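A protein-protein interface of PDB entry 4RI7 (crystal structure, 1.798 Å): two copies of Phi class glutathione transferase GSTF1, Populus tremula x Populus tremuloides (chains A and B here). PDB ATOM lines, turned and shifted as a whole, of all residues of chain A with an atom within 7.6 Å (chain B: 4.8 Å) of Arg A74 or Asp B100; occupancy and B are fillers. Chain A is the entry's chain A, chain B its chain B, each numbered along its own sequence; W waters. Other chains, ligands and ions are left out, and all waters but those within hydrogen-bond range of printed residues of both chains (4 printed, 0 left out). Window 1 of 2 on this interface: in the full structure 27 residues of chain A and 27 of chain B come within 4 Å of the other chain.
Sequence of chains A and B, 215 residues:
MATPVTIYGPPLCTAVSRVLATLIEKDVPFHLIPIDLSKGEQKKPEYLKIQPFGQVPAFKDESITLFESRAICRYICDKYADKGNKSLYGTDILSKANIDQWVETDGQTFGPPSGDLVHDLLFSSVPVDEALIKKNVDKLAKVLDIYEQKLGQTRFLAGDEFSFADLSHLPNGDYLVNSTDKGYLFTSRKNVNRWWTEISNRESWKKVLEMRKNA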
ATOM      1  N   THR A  22       5.346  33.622 -37.366  1.00  0.00           N
ATOM      2  CA  THR A  22       4.132  33.947 -36.601  1.00  0.00           C
ATOM      3  C   THR A  22       4.150  35.387 -36.057  1.00  0.00           C
ATOM      4  O   THR A  22       3.161  36.136 -36.198  1.00  0.00           O
ATOM      5  CB  THR A  22       3.945  32.936 -35.457  1.00  0.00           C
ATOM      6  OG1 THR A  22       3.934  31.602 -36.005  1.00  0.00           O
ATOM      7  CG2 THR A  22       2.646  33.217 -34.692  1.00  0.00           C
ATOM      8  N   LEU A  66       8.510  31.296 -22.123  1.00  0.00           N
ATOM      9  CA  LEU A  66       7.943  30.114 -22.748  1.00  0.00           C
ATOM     10  C   LEU A  66       8.944  29.440 -23.662  1.00  0.00           C
ATOM     11  O   LEU A  66       9.799  30.104 -24.231  1.00  0.00           O
ATOM     12  CB  LEU A  66       6.701  30.463 -23.563  1.00  0.00           C
ATOM     13  CG  LEU A  66       5.447  30.940 -22.834  1.00  0.00           C
ATOM     14  CD1 LEU A  66       4.501  31.523 -23.824  1.00  0.00           C
ATOM     15  CD2 LEU A  66       4.751  29.846 -22.016  1.00  0.00           C
ATOM     16  N   PHE A  67       8.828  28.121 -23.811  1.00  0.00           N
ATOM     17  CA  PHE A  67       9.554  27.423 -24.868  1.00  0.00           C
ATOM     18  C   PHE A  67       8.610  26.442 -25.591  1.00  0.00           C
ATOM     19  O   PHE A  67       7.426  26.392 -25.286  1.00  0.00           O
ATOM     20  CB  PHE A  67      10.781  26.722 -24.284  1.00  0.00           C
ATOM     21  CG  PHE A  67      10.452  25.696 -23.231  1.00  0.00           C
ATOM     22  CD1 PHE A  67      10.328  26.061 -21.898  1.00  0.00           C
ATOM     23  CD2 PHE A  67      10.269  24.359 -23.567  1.00  0.00           C
ATOM     24  CE1 PHE A  67      10.012  25.101 -20.913  1.00  0.00           C
ATOM     25  CE2 PHE A  67       9.953  23.397 -22.581  1.00  0.00           C
ATOM     26  CZ  PHE A  67       9.826  23.772 -21.266  1.00  0.00           C
ATOM     27  N   GLU A  68       9.163  25.684 -26.536  1.00  0.00           N
ATOM     28  CA  GLU A  68       8.417  24.931 -27.555  1.00  0.00           C
ATOM     29  C   GLU A  68       7.720  25.861 -28.551  1.00  0.00           C
ATOM     30  O   GLU A  68       6.773  26.567 -28.223  1.00  0.00           O
ATOM     31  CB  GLU A  68       7.403  23.973 -26.932  1.00  0.00           C
ATOM     32  CG  GLU A  68       8.090  22.673 -26.446  1.00  0.00           C
ATOM     33  CD  GLU A  68       8.574  21.769 -27.581  1.00  0.00           C
ATOM     34  OE1 GLU A  68       8.260  22.020 -28.772  1.00  0.00           O
ATOM     35  OE2 GLU A  68       9.253  20.780 -27.258  1.00  0.00           O
ATOM     36  N   SER A  69       8.192  25.816 -29.788  1.00  0.00           N
ATOM     37  CA  SER A  69       7.800  26.806 -30.794  1.00  0.00           C
ATOM     38  C   SER A  69       6.283  26.886 -30.967  1.00  0.00           C
ATOM     39  O   SER A  69       5.759  27.986 -31.075  1.00  0.00           O
ATOM     40  CB  SER A  69       8.482  26.486 -32.133  1.00  0.00           C
ATOM     41  OG  SER A  69       8.140  25.176 -32.583  1.00  0.00           O
ATOM     42  N   ARG A  70       5.572  25.758 -30.928  1.00  0.00           N
ATOM     43  CA  ARG A  70       4.130  25.784 -31.197  1.00  0.00           C
ATOM     44  C   ARG A  70       3.341  26.374 -30.018  1.00  0.00           C
ATOM     45  O   ARG A  70       2.296  27.017 -30.208  1.00  0.00           O
ATOM     46  CB  ARG A  70       3.593  24.392 -31.537  1.00  0.00           C
ATOM     47  CG  ARG A  70       4.041  23.889 -32.915  1.00  0.00           C
ATOM     48  CD  ARG A  70       3.830  22.393 -33.081  1.00  0.00           C
ATOM     49  NE  ARG A  70       4.486  21.919 -34.308  1.00  0.00           N
ATOM     50  CZ  ARG A  70       5.779  21.592 -34.393  1.00  0.00           C
ATOM     51  NH1 ARG A  70       6.580  21.678 -33.343  1.00  0.00           N
ATOM     52  NH2 ARG A  70       6.283  21.179 -35.532  1.00  0.00           N
ATOM     53  N   ALA A  71       3.838  26.141 -28.807  1.00  0.00           N
ATOM     54  CA  ALA A  71       3.242  26.752 -27.631  1.00  0.00           C
ATOM     55  C   ALA A  71       3.510  28.253 -27.662  1.00  0.00           C
ATOM     56  O   ALA A  71       2.632  29.060 -27.336  1.00  0.00           O
ATOM     57  CB  ALA A  71       3.797  26.116 -26.346  1.00  0.00           C
ATOM     58  N   ILE A  72       4.745  28.630 -27.986  1.00  0.00           N
ATOM     59  CA  ILE A  72       5.062  30.036 -28.117  1.00  0.00           C
ATOM     60  C   ILE A  72       4.085  30.688 -29.111  1.00  0.00           C
ATOM     61  O   ILE A  72       3.569  31.784 -28.859  1.00  0.00           O
ATOM     62  CB  ILE A  72       6.508  30.260 -28.578  1.00  0.00           C
ATOM     63  CG1 ILE A  72       7.500  29.875 -27.471  1.00  0.00           C
ATOM     64  CG2 ILE A  72       6.743  31.691 -28.984  1.00  0.00           C
ATOM     65  CD1 ILE A  72       8.939  29.738 -27.957  1.00  0.00           C
ATOM     66  N   CYS A  73       3.864  30.039 -30.250  1.00  0.00           N
ATOM     67  CA  CYS A  73       2.998  30.612 -31.271  1.00  0.00           C
ATOM     68  C   CYS A  73       1.537  30.663 -30.812  1.00  0.00           C
ATOM     69  O   CYS A  73       0.835  31.623 -31.148  1.00  0.00           O
ATOM     70  CB  CYS A  73       3.119  29.837 -32.585  1.00  0.00           C
ATOM     71  SG  CYS A  73       4.757  30.001 -33.326  1.00  0.00           S
ATOM     72  N   ARG A  74       1.062  29.673 -30.049  1.00  0.00           N
ATOM     73  CA  ARG A  74      -0.342  29.732 -29.626  1.00  0.00           C
ATOM     74  C   ARG A  74      -0.547  30.905 -28.661  1.00  0.00           C
ATOM     75  O   ARG A  74      -1.557  31.612 -28.732  1.00  0.00           O
ATOM     76  CB  ARG A  74      -0.831  28.413 -29.001  1.00  0.00           C
ATOM     77  CG  ARG A  74      -1.432  27.465 -30.070  1.00  0.00           C
ATOM     78  CD  ARG A  74      -2.124  26.212 -29.528  1.00  0.00           C
ATOM     79  NE  ARG A  74      -1.190  25.335 -28.879  1.00  0.00           N
ATOM     80  CZ  ARG A  74      -0.528  24.321 -29.433  1.00  0.00           C
ATOM     81  NH1 ARG A  74      -0.688  23.978 -30.709  1.00  0.00           N
ATOM     82  NH2 ARG A  74       0.301  23.620 -28.669  1.00  0.00           N
ATOM     83  N   TYR A  75       0.429  31.122 -27.795  1.00  0.00           N
ATOM     84  CA  TYR A  75       0.404  32.247 -26.889  1.00  0.00           C
ATOM     85  C   TYR A  75       0.362  33.584 -27.633  1.00  0.00           C
ATOM     86  O   TYR A  75      -0.413  34.482 -27.282  1.00  0.00           O
ATOM     87  CB  TYR A  75       1.622  32.207 -25.981  1.00  0.00           C
ATOM     88  CG  TYR A  75       1.694  33.401 -25.052  1.00  0.00           C
ATOM     89  CD1 TYR A  75       0.736  33.611 -24.067  1.00  0.00           C
ATOM     90  CD2 TYR A  75       2.729  34.314 -25.165  1.00  0.00           C
ATOM     91  CE1 TYR A  75       0.815  34.705 -23.225  1.00  0.00           C
ATOM     92  CE2 TYR A  75       2.811  35.392 -24.343  1.00  0.00           C
ATOM     93  CZ  TYR A  75       1.861  35.598 -23.374  1.00  0.00           C
ATOM     94  OH  TYR A  75       1.985  36.707 -22.565  1.00  0.00           O
ATOM     95  N   ILE A  76       1.225  33.719 -28.628  1.00  0.00           N
ATOM     96  CA  ILE A  76       1.272  34.932 -29.450  1.00  0.00           C
ATOM     97  C   ILE A  76      -0.097  35.168 -30.118  1.00  0.00           C
ATOM     98  O   ILE A  76      -0.636  36.281 -30.094  1.00  0.00           O
ATOM     99  CB  ILE A  76       2.395  34.845 -30.532  1.00  0.00           C
ATOM    100  CG1 ILE A  76       3.780  34.890 -29.864  1.00  0.00           C
ATOM    101  CG2 ILE A  76       2.282  35.986 -31.572  1.00  0.00           C
ATOM    102  CD1 ILE A  76       4.905  34.393 -30.766  1.00  0.00           C
ATOM    103  N   CYS A  77      -0.666  34.119 -30.706  1.00  0.00           N
ATOM    104  CA  CYS A  77      -1.975  34.256 -31.366  1.00  0.00           C
ATOM    105  C   CYS A  77      -3.101  34.608 -30.408  1.00  0.00           C
ATOM    106  O   CYS A  77      -4.070  35.254 -30.788  1.00  0.00           O
ATOM    107  CB  CYS A  77      -2.312  32.970 -32.126  1.00  0.00           C
ATOM    108  SG  CYS A  77      -1.292  32.776 -33.601  1.00  0.00           S
ATOM    109  N   ASP A  78      -2.951  34.162 -29.171  1.00  0.00           N
ATOM    110  CA  ASP A  78      -3.863  34.433 -28.082  1.00  0.00           C
ATOM    111  C   ASP A  78      -3.684  35.860 -27.595  1.00  0.00           C
ATOM    112  O   ASP A  78      -4.621  36.661 -27.600  1.00  0.00           O
ATOM    113  CB  ASP A  78      -3.591  33.424 -26.953  1.00  0.00           C
ATOM    114  CG  ASP A  78      -4.828  32.986 -26.217  1.00  0.00           C
ATOM    115  OD1 ASP A  78      -5.756  33.812 -26.047  1.00  0.00           O
ATOM    116  OD2 ASP A  78      -4.850  31.802 -25.784  1.00  0.00           O
ATOM    117  N   LYS A  79      -2.475  36.197 -27.179  1.00  0.00           N
ATOM    118  CA  LYS A  79      -2.244  37.523 -26.599  1.00  0.00           C
ATOM    119  C   LYS A  79      -2.514  38.653 -27.624  1.00  0.00           C
ATOM    120  O   LYS A  79      -3.043  39.720 -27.294  1.00  0.00           O
ATOM    121  CB  LYS A  79      -0.809  37.606 -26.082  1.00  0.00           C
ATOM    122  CG  LYS A  79      -0.409  38.971 -25.511  1.00  0.00           C
ATOM    123  CD  LYS A  79       1.033  38.984 -24.989  1.00  0.00           C
ATOM    124  CE  LYS A  79       1.408  40.289 -24.316  1.00  0.00           C
ATOM    125  NZ  LYS A  79       2.870  40.480 -24.313  1.00  0.00           N
ATOM    126  N   TYR A  80      -2.138  38.418 -28.868  1.00  0.00           N
ATOM    127  CA  TYR A  80      -2.261  39.436 -29.930  1.00  0.00           C
ATOM    128  C   TYR A  80      -3.366  39.090 -30.917  1.00  0.00           C
ATOM    129  O   TYR A  80      -3.259  39.363 -32.120  1.00  0.00           O
ATOM    130  CB  TYR A  80      -0.916  39.579 -30.673  1.00  0.00           C
ATOM    131  CG  TYR A  80       0.222  39.975 -29.759  1.00  0.00           C
ATOM    132  CD1 TYR A  80       0.408  41.303 -29.384  1.00  0.00           C
ATOM    133  CD2 TYR A  80       1.090  39.016 -29.243  1.00  0.00           C
ATOM    134  CE1 TYR A  80       1.438  41.670 -28.531  1.00  0.00           C
ATOM    135  CE2 TYR A  80       2.122  39.378 -28.392  1.00  0.00           C
ATOM    136  CZ  TYR A  80       2.291  40.702 -28.041  1.00  0.00           C
ATOM    137  OH  TYR A  80       3.315  41.053 -27.202  1.00  0.00           O
ATOM    138  N   TYR A  89      -5.095  31.767 -36.216  1.00  0.00           N
ATOM    139  CA  TYR A  89      -5.397  30.559 -35.436  1.00  0.00           C
ATOM    140  C   TYR A  89      -6.886  30.545 -35.070  1.00  0.00           C
ATOM    141  O   TYR A  89      -7.303  30.044 -34.017  1.00  0.00           O
ATOM    142  CB  TYR A  89      -4.498  30.464 -34.195  1.00  0.00           C
ATOM    143  CG  TYR A  89      -4.034  29.064 -33.828  1.00  0.00           C
ATOM    144  CD1 TYR A  89      -4.918  27.991 -33.691  1.00  0.00           C
ATOM    145  CD2 TYR A  89      -2.677  28.816 -33.617  1.00  0.00           C
ATOM    146  CE1 TYR A  89      -4.446  26.714 -33.361  1.00  0.00           C
ATOM    147  CE2 TYR A  89      -2.210  27.576 -33.303  1.00  0.00           C
ATOM    148  CZ  TYR A  89      -3.079  26.523 -33.171  1.00  0.00           C
ATOM    149  OH  TYR A  89      -2.537  25.324 -32.813  1.00  0.00           O
ATOM    150  N   LYS A  96     -10.883  27.587 -34.159  1.00  0.00           N
ATOM    151  CA  LYS A  96      -9.598  27.298 -33.544  1.00  0.00           C
ATOM    152  C   LYS A  96      -9.292  25.777 -33.526  1.00  0.00           C
ATOM    153  O   LYS A  96      -8.192  25.364 -33.891  1.00  0.00           O
ATOM    154  CB  LYS A  96      -9.536  27.858 -32.117  1.00  0.00           C
ATOM    155  CG  LYS A  96      -8.187  27.586 -31.454  1.00  0.00           C
ATOM    156  CD  LYS A  96      -8.046  28.208 -30.073  1.00  0.00           C
ATOM    157  CE  LYS A  96      -6.640  27.949 -29.527  1.00  0.00           C
ATOM    158  NZ  LYS A  96      -6.362  28.714 -28.287  1.00  0.00           N
ATOM    159  N   ASP A 100      -6.475  23.517 -35.294  1.00  0.00           N
ATOM    160  CA  ASP A 100      -5.558  22.914 -34.349  1.00  0.00           C
ATOM    161  C   ASP A 100      -5.275  21.452 -34.697  1.00  0.00           C
ATOM    162  O   ASP A 100      -4.171  20.954 -34.450  1.00  0.00           O
ATOM    163  CB  ASP A 100      -6.113  23.036 -32.926  1.00  0.00           C
ATOM    164  CG  ASP A 100      -5.072  22.722 -31.845  1.00  0.00           C
ATOM    165  OD1 ASP A 100      -3.905  23.180 -31.930  1.00  0.00           O
ATOM    166  OD2 ASP A 100      -5.437  21.999 -30.901  1.00  0.00           O
ATOM    167  N   VAL A 103      -2.576  21.452 -37.028  1.00  0.00           N
ATOM    168  CA  VAL A 103      -1.362  21.833 -36.348  1.00  0.00           C
ATOM    169  C   VAL A 103      -0.757  20.595 -35.670  1.00  0.00           C
ATOM    170  O   VAL A 103       0.463  20.390 -35.707  1.00  0.00           O
ATOM    171  CB  VAL A 103      -1.605  22.957 -35.328  1.00  0.00           C
ATOM    172  CG1 VAL A 103      -0.292  23.310 -34.587  1.00  0.00           C
ATOM    173  CG2 VAL A 103      -2.152  24.172 -36.008  1.00  0.00           C
ATOM    174  N   GLU A 104      -1.617  19.751 -35.097  1.00  0.00           N
ATOM    175  CA  GLU A 104      -1.164  18.508 -34.485  1.00  0.00           C
ATOM    176  C   GLU A 104      -0.656  17.523 -35.525  1.00  0.00           C
ATOM    177  O   GLU A 104       0.241  16.726 -35.258  1.00  0.00           O
ATOM    178  CB  GLU A 104      -2.296  17.879 -33.689  1.00  0.00           C
ATOM    179  CG  GLU A 104      -2.502  18.548 -32.346  1.00  0.00           C
ATOM    180  CD  GLU A 104      -1.278  18.444 -31.442  1.00  0.00           C
ATOM    181  OE1 GLU A 104      -0.691  17.338 -31.324  1.00  0.00           O
ATOM    182  OE2 GLU A 104      -0.896  19.487 -30.838  1.00  0.00           O
ATOM    183  N   PHE A 164      -2.347  28.951 -39.127  1.00  0.00           N
ATOM    184  CA  PHE A 164      -1.128  28.466 -38.487  1.00  0.00           C
ATOM    185  C   PHE A 164      -0.789  27.016 -38.845  1.00  0.00           C
ATOM    186  O   PHE A 164       0.378  26.572 -38.734  1.00  0.00           O
ATOM    187  CB  PHE A 164      -1.253  28.588 -36.981  1.00  0.00           C
ATOM    188  CG  PHE A 164       0.002  28.254 -36.276  1.00  0.00           C
ATOM    189  CD1 PHE A 164       1.067  29.130 -36.317  1.00  0.00           C
ATOM    190  CD2 PHE A 164       0.158  27.040 -35.662  1.00  0.00           C
ATOM    191  CE1 PHE A 164       2.256  28.819 -35.690  1.00  0.00           C
ATOM    192  CE2 PHE A 164       1.339  26.717 -35.049  1.00  0.00           C
ATOM    193  CZ  PHE A 164       2.393  27.603 -35.060  1.00  0.00           C
ATOM    194  N   ARG B  74      -7.687  19.699 -26.429  1.00  0.00           N
ATOM    195  CA  ARG B  74      -7.738  21.150 -26.278  1.00  0.00           C
ATOM    196  C   ARG B  74      -9.162  21.682 -26.537  1.00  0.00           C
ATOM    197  O   ARG B  74      -9.664  22.553 -25.822  1.00  0.00           O
ATOM    198  CB  ARG B  74      -6.724  21.832 -27.199  1.00  0.00           C
ATOM    199  CG  ARG B  74      -5.364  22.009 -26.532  1.00  0.00           C
ATOM    200  CD  ARG B  74      -4.466  23.001 -27.270  1.00  0.00           C
ATOM    201  NE  ARG B  74      -4.015  22.421 -28.522  1.00  0.00           N
ATOM    202  CZ  ARG B  74      -2.951  21.631 -28.672  1.00  0.00           C
ATOM    203  NH1 ARG B  74      -2.708  21.159 -29.856  1.00  0.00           N
ATOM    204  NH2 ARG B  74      -2.124  21.331 -27.672  1.00  0.00           N
ATOM    205  N   TYR B  89      -6.503  22.816 -18.233  1.00  0.00           N
ATOM    206  CA  TYR B  89      -5.675  23.472 -19.240  1.00  0.00           C
ATOM    207  C   TYR B  89      -5.665  24.976 -18.971  1.00  0.00           C
ATOM    208  O   TYR B  89      -5.694  25.790 -19.890  1.00  0.00           O
ATOM    209  CB  TYR B  89      -6.186  23.139 -20.655  1.00  0.00           C
ATOM    210  CG  TYR B  89      -5.109  22.900 -21.710  1.00  0.00           C
ATOM    211  CD1 TYR B  89      -4.047  23.783 -21.904  1.00  0.00           C
ATOM    212  CD2 TYR B  89      -5.169  21.769 -22.510  1.00  0.00           C
ATOM    213  CE1 TYR B  89      -3.085  23.544 -22.884  1.00  0.00           C
ATOM    214  CE2 TYR B  89      -4.210  21.510 -23.460  1.00  0.00           C
ATOM    215  CZ  TYR B  89      -3.178  22.387 -23.651  1.00  0.00           C
ATOM    216  OH  TYR B  89      -2.267  22.092 -24.629  1.00  0.00           O
ATOM    217  N   LYS B  96      -2.775  28.949 -19.359  1.00  0.00           N
ATOM    218  CA  LYS B  96      -2.925  28.006 -20.462  1.00  0.00           C
ATOM    219  C   LYS B  96      -1.593  27.820 -21.192  1.00  0.00           C
ATOM    220  O   LYS B  96      -1.198  26.691 -21.471  1.00  0.00           O
ATOM    221  CB  LYS B  96      -4.001  28.475 -21.459  1.00  0.00           C
ATOM    222  CG  LYS B  96      -4.188  27.512 -22.651  1.00  0.00           C
ATOM    223  CD  LYS B  96      -5.015  28.119 -23.781  1.00  0.00           C
ATOM    224  CE  LYS B  96      -6.441  28.444 -23.352  1.00  0.00           C
ATOM    225  NZ  LYS B  96      -7.212  29.158 -24.418  1.00  0.00           N
ATOM    226  N   ALA B  97      -0.919  28.930 -21.504  1.00  0.00           N
ATOM    227  CA  ALA B  97       0.336  28.871 -22.259  1.00  0.00           C
ATOM    228  C   ALA B  97       1.389  28.158 -21.431  1.00  0.00           C
ATOM    229  O   ALA B  97       2.153  27.382 -21.958  1.00  0.00           O
ATOM    230  CB  ALA B  97       0.810  30.241 -22.641  1.00  0.00           C
ATOM    231  N   ASN B  98       1.392  28.419 -20.123  1.00  0.00           N
ATOM    232  CA  ASN B  98       2.375  27.812 -19.243  1.00  0.00           C
ATOM    233  C   ASN B  98       2.230  26.282 -19.241  1.00  0.00           C
ATOM    234  O   ASN B  98       3.226  25.561 -19.214  1.00  0.00           O
ATOM    235  CB  ASN B  98       2.270  28.376 -17.814  1.00  0.00           C
ATOM    236  CG  ASN B  98       3.122  27.599 -16.830  1.00  0.00           C
ATOM    237  OD1 ASN B  98       4.339  27.482 -17.010  1.00  0.00           O
ATOM    238  ND2 ASN B  98       2.489  27.008 -15.830  1.00  0.00           N
ATOM    239  N   ILE B  99       0.996  25.796 -19.265  1.00  0.00           N
ATOM    240  CA  ILE B  99       0.734  24.372 -19.362  1.00  0.00           C
ATOM    241  C   ILE B  99       1.111  23.870 -20.773  1.00  0.00           C
ATOM    242  O   ILE B  99       1.725  22.805 -20.942  1.00  0.00           O
ATOM    243  CB  ILE B  99      -0.772  24.061 -19.039  1.00  0.00           C
ATOM    244  CG1 ILE B  99      -1.031  24.228 -17.538  1.00  0.00           C
ATOM    245  CG2 ILE B  99      -1.183  22.640 -19.465  1.00  0.00           C
ATOM    246  CD1 ILE B  99      -2.497  24.433 -17.169  1.00  0.00           C
ATOM    247  N   ASP B 100       0.755  24.671 -21.775  1.00  0.00           N
ATOM    248  CA  ASP B 100       0.897  24.282 -23.177  1.00  0.00           C
ATOM    249  C   ASP B 100       2.349  23.945 -23.562  1.00  0.00           C
ATOM    250  O   ASP B 100       2.601  23.029 -24.362  1.00  0.00           O
ATOM    251  CB  ASP B 100       0.349  25.406 -24.072  1.00  0.00           C
ATOM    252  CG  ASP B 100      -0.020  24.928 -25.486  1.00  0.00           C
ATOM    253  OD1 ASP B 100      -0.535  23.795 -25.655  1.00  0.00           O
ATOM    254  OD2 ASP B 100       0.197  25.715 -26.419  1.00  0.00           O
ATOM    255  N   GLN B 101       3.313  24.674 -23.022  1.00  0.00           N
ATOM    256  CA  GLN B 101       4.712  24.400 -23.387  1.00  0.00           C
ATOM    257  C   GLN B 101       5.124  22.980 -22.963  1.00  0.00           C
ATOM    258  O   GLN B 101       5.884  22.317 -23.663  1.00  0.00           O
ATOM    259  CB  GLN B 101       5.657  25.441 -22.778  1.00  0.00           C
ATOM    260  CG  GLN B 101       5.771  25.408 -21.243  1.00  0.00           C
ATOM    261  CD  GLN B 101       6.480  26.635 -20.701  1.00  0.00           C
ATOM    262  OE1 GLN B 101       7.398  27.184 -21.335  1.00  0.00           O
ATOM    263  NE2 GLN B 101       6.081  27.062 -19.519  1.00  0.00           N
ATOM    264  N   TRP B 102       4.554  22.498 -21.859  1.00  0.00           N
ATOM    265  CA  TRP B 102       4.857  21.159 -21.350  1.00  0.00           C
ATOM    266  C   TRP B 102       4.013  20.132 -22.069  1.00  0.00           C
ATOM    267  O   TRP B 102       4.402  18.978 -22.141  1.00  0.00           O
ATOM    268  CB  TRP B 102       4.661  21.087 -19.820  1.00  0.00           C
ATOM    269  CG  TRP B 102       5.741  21.855 -19.104  1.00  0.00           C
ATOM    270  CD1 TRP B 102       5.637  23.098 -18.553  1.00  0.00           C
ATOM    271  CD2 TRP B 102       7.110  21.435 -18.888  1.00  0.00           C
ATOM    272  NE1 TRP B 102       6.855  23.491 -18.024  1.00  0.00           N
ATOM    273  CE2 TRP B 102       7.773  22.492 -18.218  1.00  0.00           C
ATOM    274  CE3 TRP B 102       7.838  20.287 -19.220  1.00  0.00           C
ATOM    275  CZ2 TRP B 102       9.122  22.428 -17.860  1.00  0.00           C
ATOM    276  CZ3 TRP B 102       9.188  20.220 -18.865  1.00  0.00           C
ATOM    277  CH2 TRP B 102       9.815  21.298 -18.192  1.00  0.00           C
ATOM    278  N   VAL B 103       2.877  20.536 -22.644  1.00  0.00           N
ATOM    279  CA  VAL B 103       2.125  19.633 -23.525  1.00  0.00           C
ATOM    280  C   VAL B 103       2.926  19.427 -24.810  1.00  0.00           C
ATOM    281  O   VAL B 103       3.014  18.312 -25.333  1.00  0.00           O
ATOM    282  CB  VAL B 103       0.708  20.176 -23.877  1.00  0.00           C
ATOM    283  CG1 VAL B 103      -0.040  19.241 -24.857  1.00  0.00           C
ATOM    284  CG2 VAL B 103      -0.134  20.385 -22.641  1.00  0.00           C
ATOM    285  N   GLU B 104       3.462  20.511 -25.356  1.00  0.00           N
ATOM    286  CA  GLU B 104       4.358  20.404 -26.506  1.00  0.00           C
ATOM    287  C   GLU B 104       5.615  19.563 -26.178  1.00  0.00           C
ATOM    288  O   GLU B 104       6.117  18.836 -27.030  1.00  0.00           O
ATOM    289  CB  GLU B 104       4.772  21.791 -26.990  1.00  0.00           C
ATOM    290  CG  GLU B 104       3.653  22.544 -27.720  1.00  0.00           C
ATOM    291  CD  GLU B 104       3.214  21.818 -28.998  1.00  0.00           C
ATOM    292  OE1 GLU B 104       4.088  21.373 -29.772  1.00  0.00           O
ATOM    293  OE2 GLU B 104       1.999  21.674 -29.240  1.00  0.00           O
HETATM  294  O   HOH W   1       0.595  28.228 -25.537  1.00  0.00           O
HETATM  295  O   HOH W   2       0.307  19.552 -28.547  1.00  0.00           O
HETATM  296  O   HOH W   3       6.334  22.780 -30.553  1.00  0.00           O
HETATM  297  O   HOH W   4       0.813  21.447 -31.560  1.00  0.00           O
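OE1 of Gln B101 is in hydrogen-bond range of N of Phe A67, 3.0 Å away. NE of Arg A74 is in salt-bridge range of OD2 of Asp B100 (2.8 Å). NH2 of Arg A74 lies within salt-bridge range of OE2 of Glu B104 (2.6 Å). OD2 of Asp A78 is in salt-bridge range of NZ of Lys B96 (3.8 Å). The guanidinium group (NE) of Arg B74 lies within salt-bridge range of the side-chain carboxylate (OD2) of Asp A100. OE2 of Glu A104 lies within salt-bridge range of NH1 of Arg B74 (2.7 Å). The guanidinium group of Arg A74 sits close to the guanidinium group of Arg B74.
The side-chain carboxylate (OD1) of Asp A100 lies within salt-bridge range of the guanidinium group (NH1) of Arg A74. NH2 of Arg B74 lies within salt-bridge range of OD1 of Asp B100, 3.6 Å away. The side-chain hydroxyl (OH) of Tyr B89 is in hydrogen-bond range of the side-chain carboxylate (OD1) of Asp B100 (2.6 Å). The side-chain amide oxygen of Asn B98 is in hydrogen-bond range of the side-chain amide nitrogen of Gln B101, at 3.1 Å.
O of Ala B97 touches CD2 of Leu A66, 3.6 Å away. Leu A66 touches Gln B101. CZ of Phe A67 touches CZ2 of Trp B102, at 3.7 Å. CG of Glu A68 touches O of Gln B101, 3.6 Å away. Glu A68 touches Glu B104. Glu B104 touches Arg A70 (OE1 to CD, 3.5 Å). Ala A71 touches Asp B100. Ala A71 touches Glu B104 (N to CG, 3.8 Å). CD1 of Tyr A75 touches CB of Ala B97 (3.7 Å). NZ of Lys B96 touches NZ of Lys A96, at 3.99 Å.
Of the printed residues of chain B, Arg A74 touches Arg B74 (3.5 Å), Asp B100 (2.8 Å) and Glu B104 (2.6 Å). Of the printed residues of chain B, Tyr A75 touches Ala B97 (3.7 Å). Of the printed residues of chain B, Lys A96 touches Lys B96 (3.99 Å). Of the printed residues of chain B, Glu A104 touches Arg B74 (2.7 Å) and Glu B104 (3.96 Å). Phe A164 touches none of the printed residues of chain B. Of chain A, only Ala A71 and Arg A74 come within 4 Å of Asp B100. The nearest residue of chain A that does not touch Asp B100 is Arg A70 (4.5 Å).
Of the 22 printed residues of chain A, 11 touch a printed residue of chain B. Of the 11 printed residues of chain B, 7 touch a printed residue of chain A. Hydrophobic or aromatic side chains of chain B within 4 Å of the printed part of chain A: Ala B97 and Trp B102. Among the printed residues, 19 pairs touch across the chains. Among the printed residues, Asp or Glu carboxylates within 4 Å of a Lys or Arg side-chain nitrogen of the other chain: Arg A74 with Asp B100 (2.8 Å), Arg A74 with Glu B104 (2.6 Å), Asp A78 with Lys B96 (3.8 Å), Asp A100 with Arg B74 (2.8 Å) and Glu A104 with Arg B74 (2.7 Å).
Arg B74 touches its own counterpart, Arg A74. Arg A74 touches Asp B100, and with the chains exchanged Asp A100 touches Arg B74. Arg A74 touches Glu B104, and with the chains exchanged Glu A104 touches Arg B74. Lys A96 touches its own counterpart, Lys B96. Positions printed for both chains: 74, 89, 96, 100, 103 and 104. Of the 19 pairs that touch across the chains among the printed residues, 7 have their exchanged pair printed and touching as well.
Water W2 lies within hydrogen-bond range of the side-chain carboxylate of Glu A104 (2.6 Å), the side-chain carboxylate of Glu B104 (2.8 Å) and the guanidinium group of Arg B74 (3.1 Å). Water W4 lies within hydrogen-bond range of OE2 of Glu B104 (2.6 Å), OE2 of Glu A104 (2.7 Å) and NH1 of Arg A74 (3.1 Å). Water W1 bridges the side-chain carboxylate (OD2) of Asp B100 and the backbone carbonyl oxygen (O) of Ala A71.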
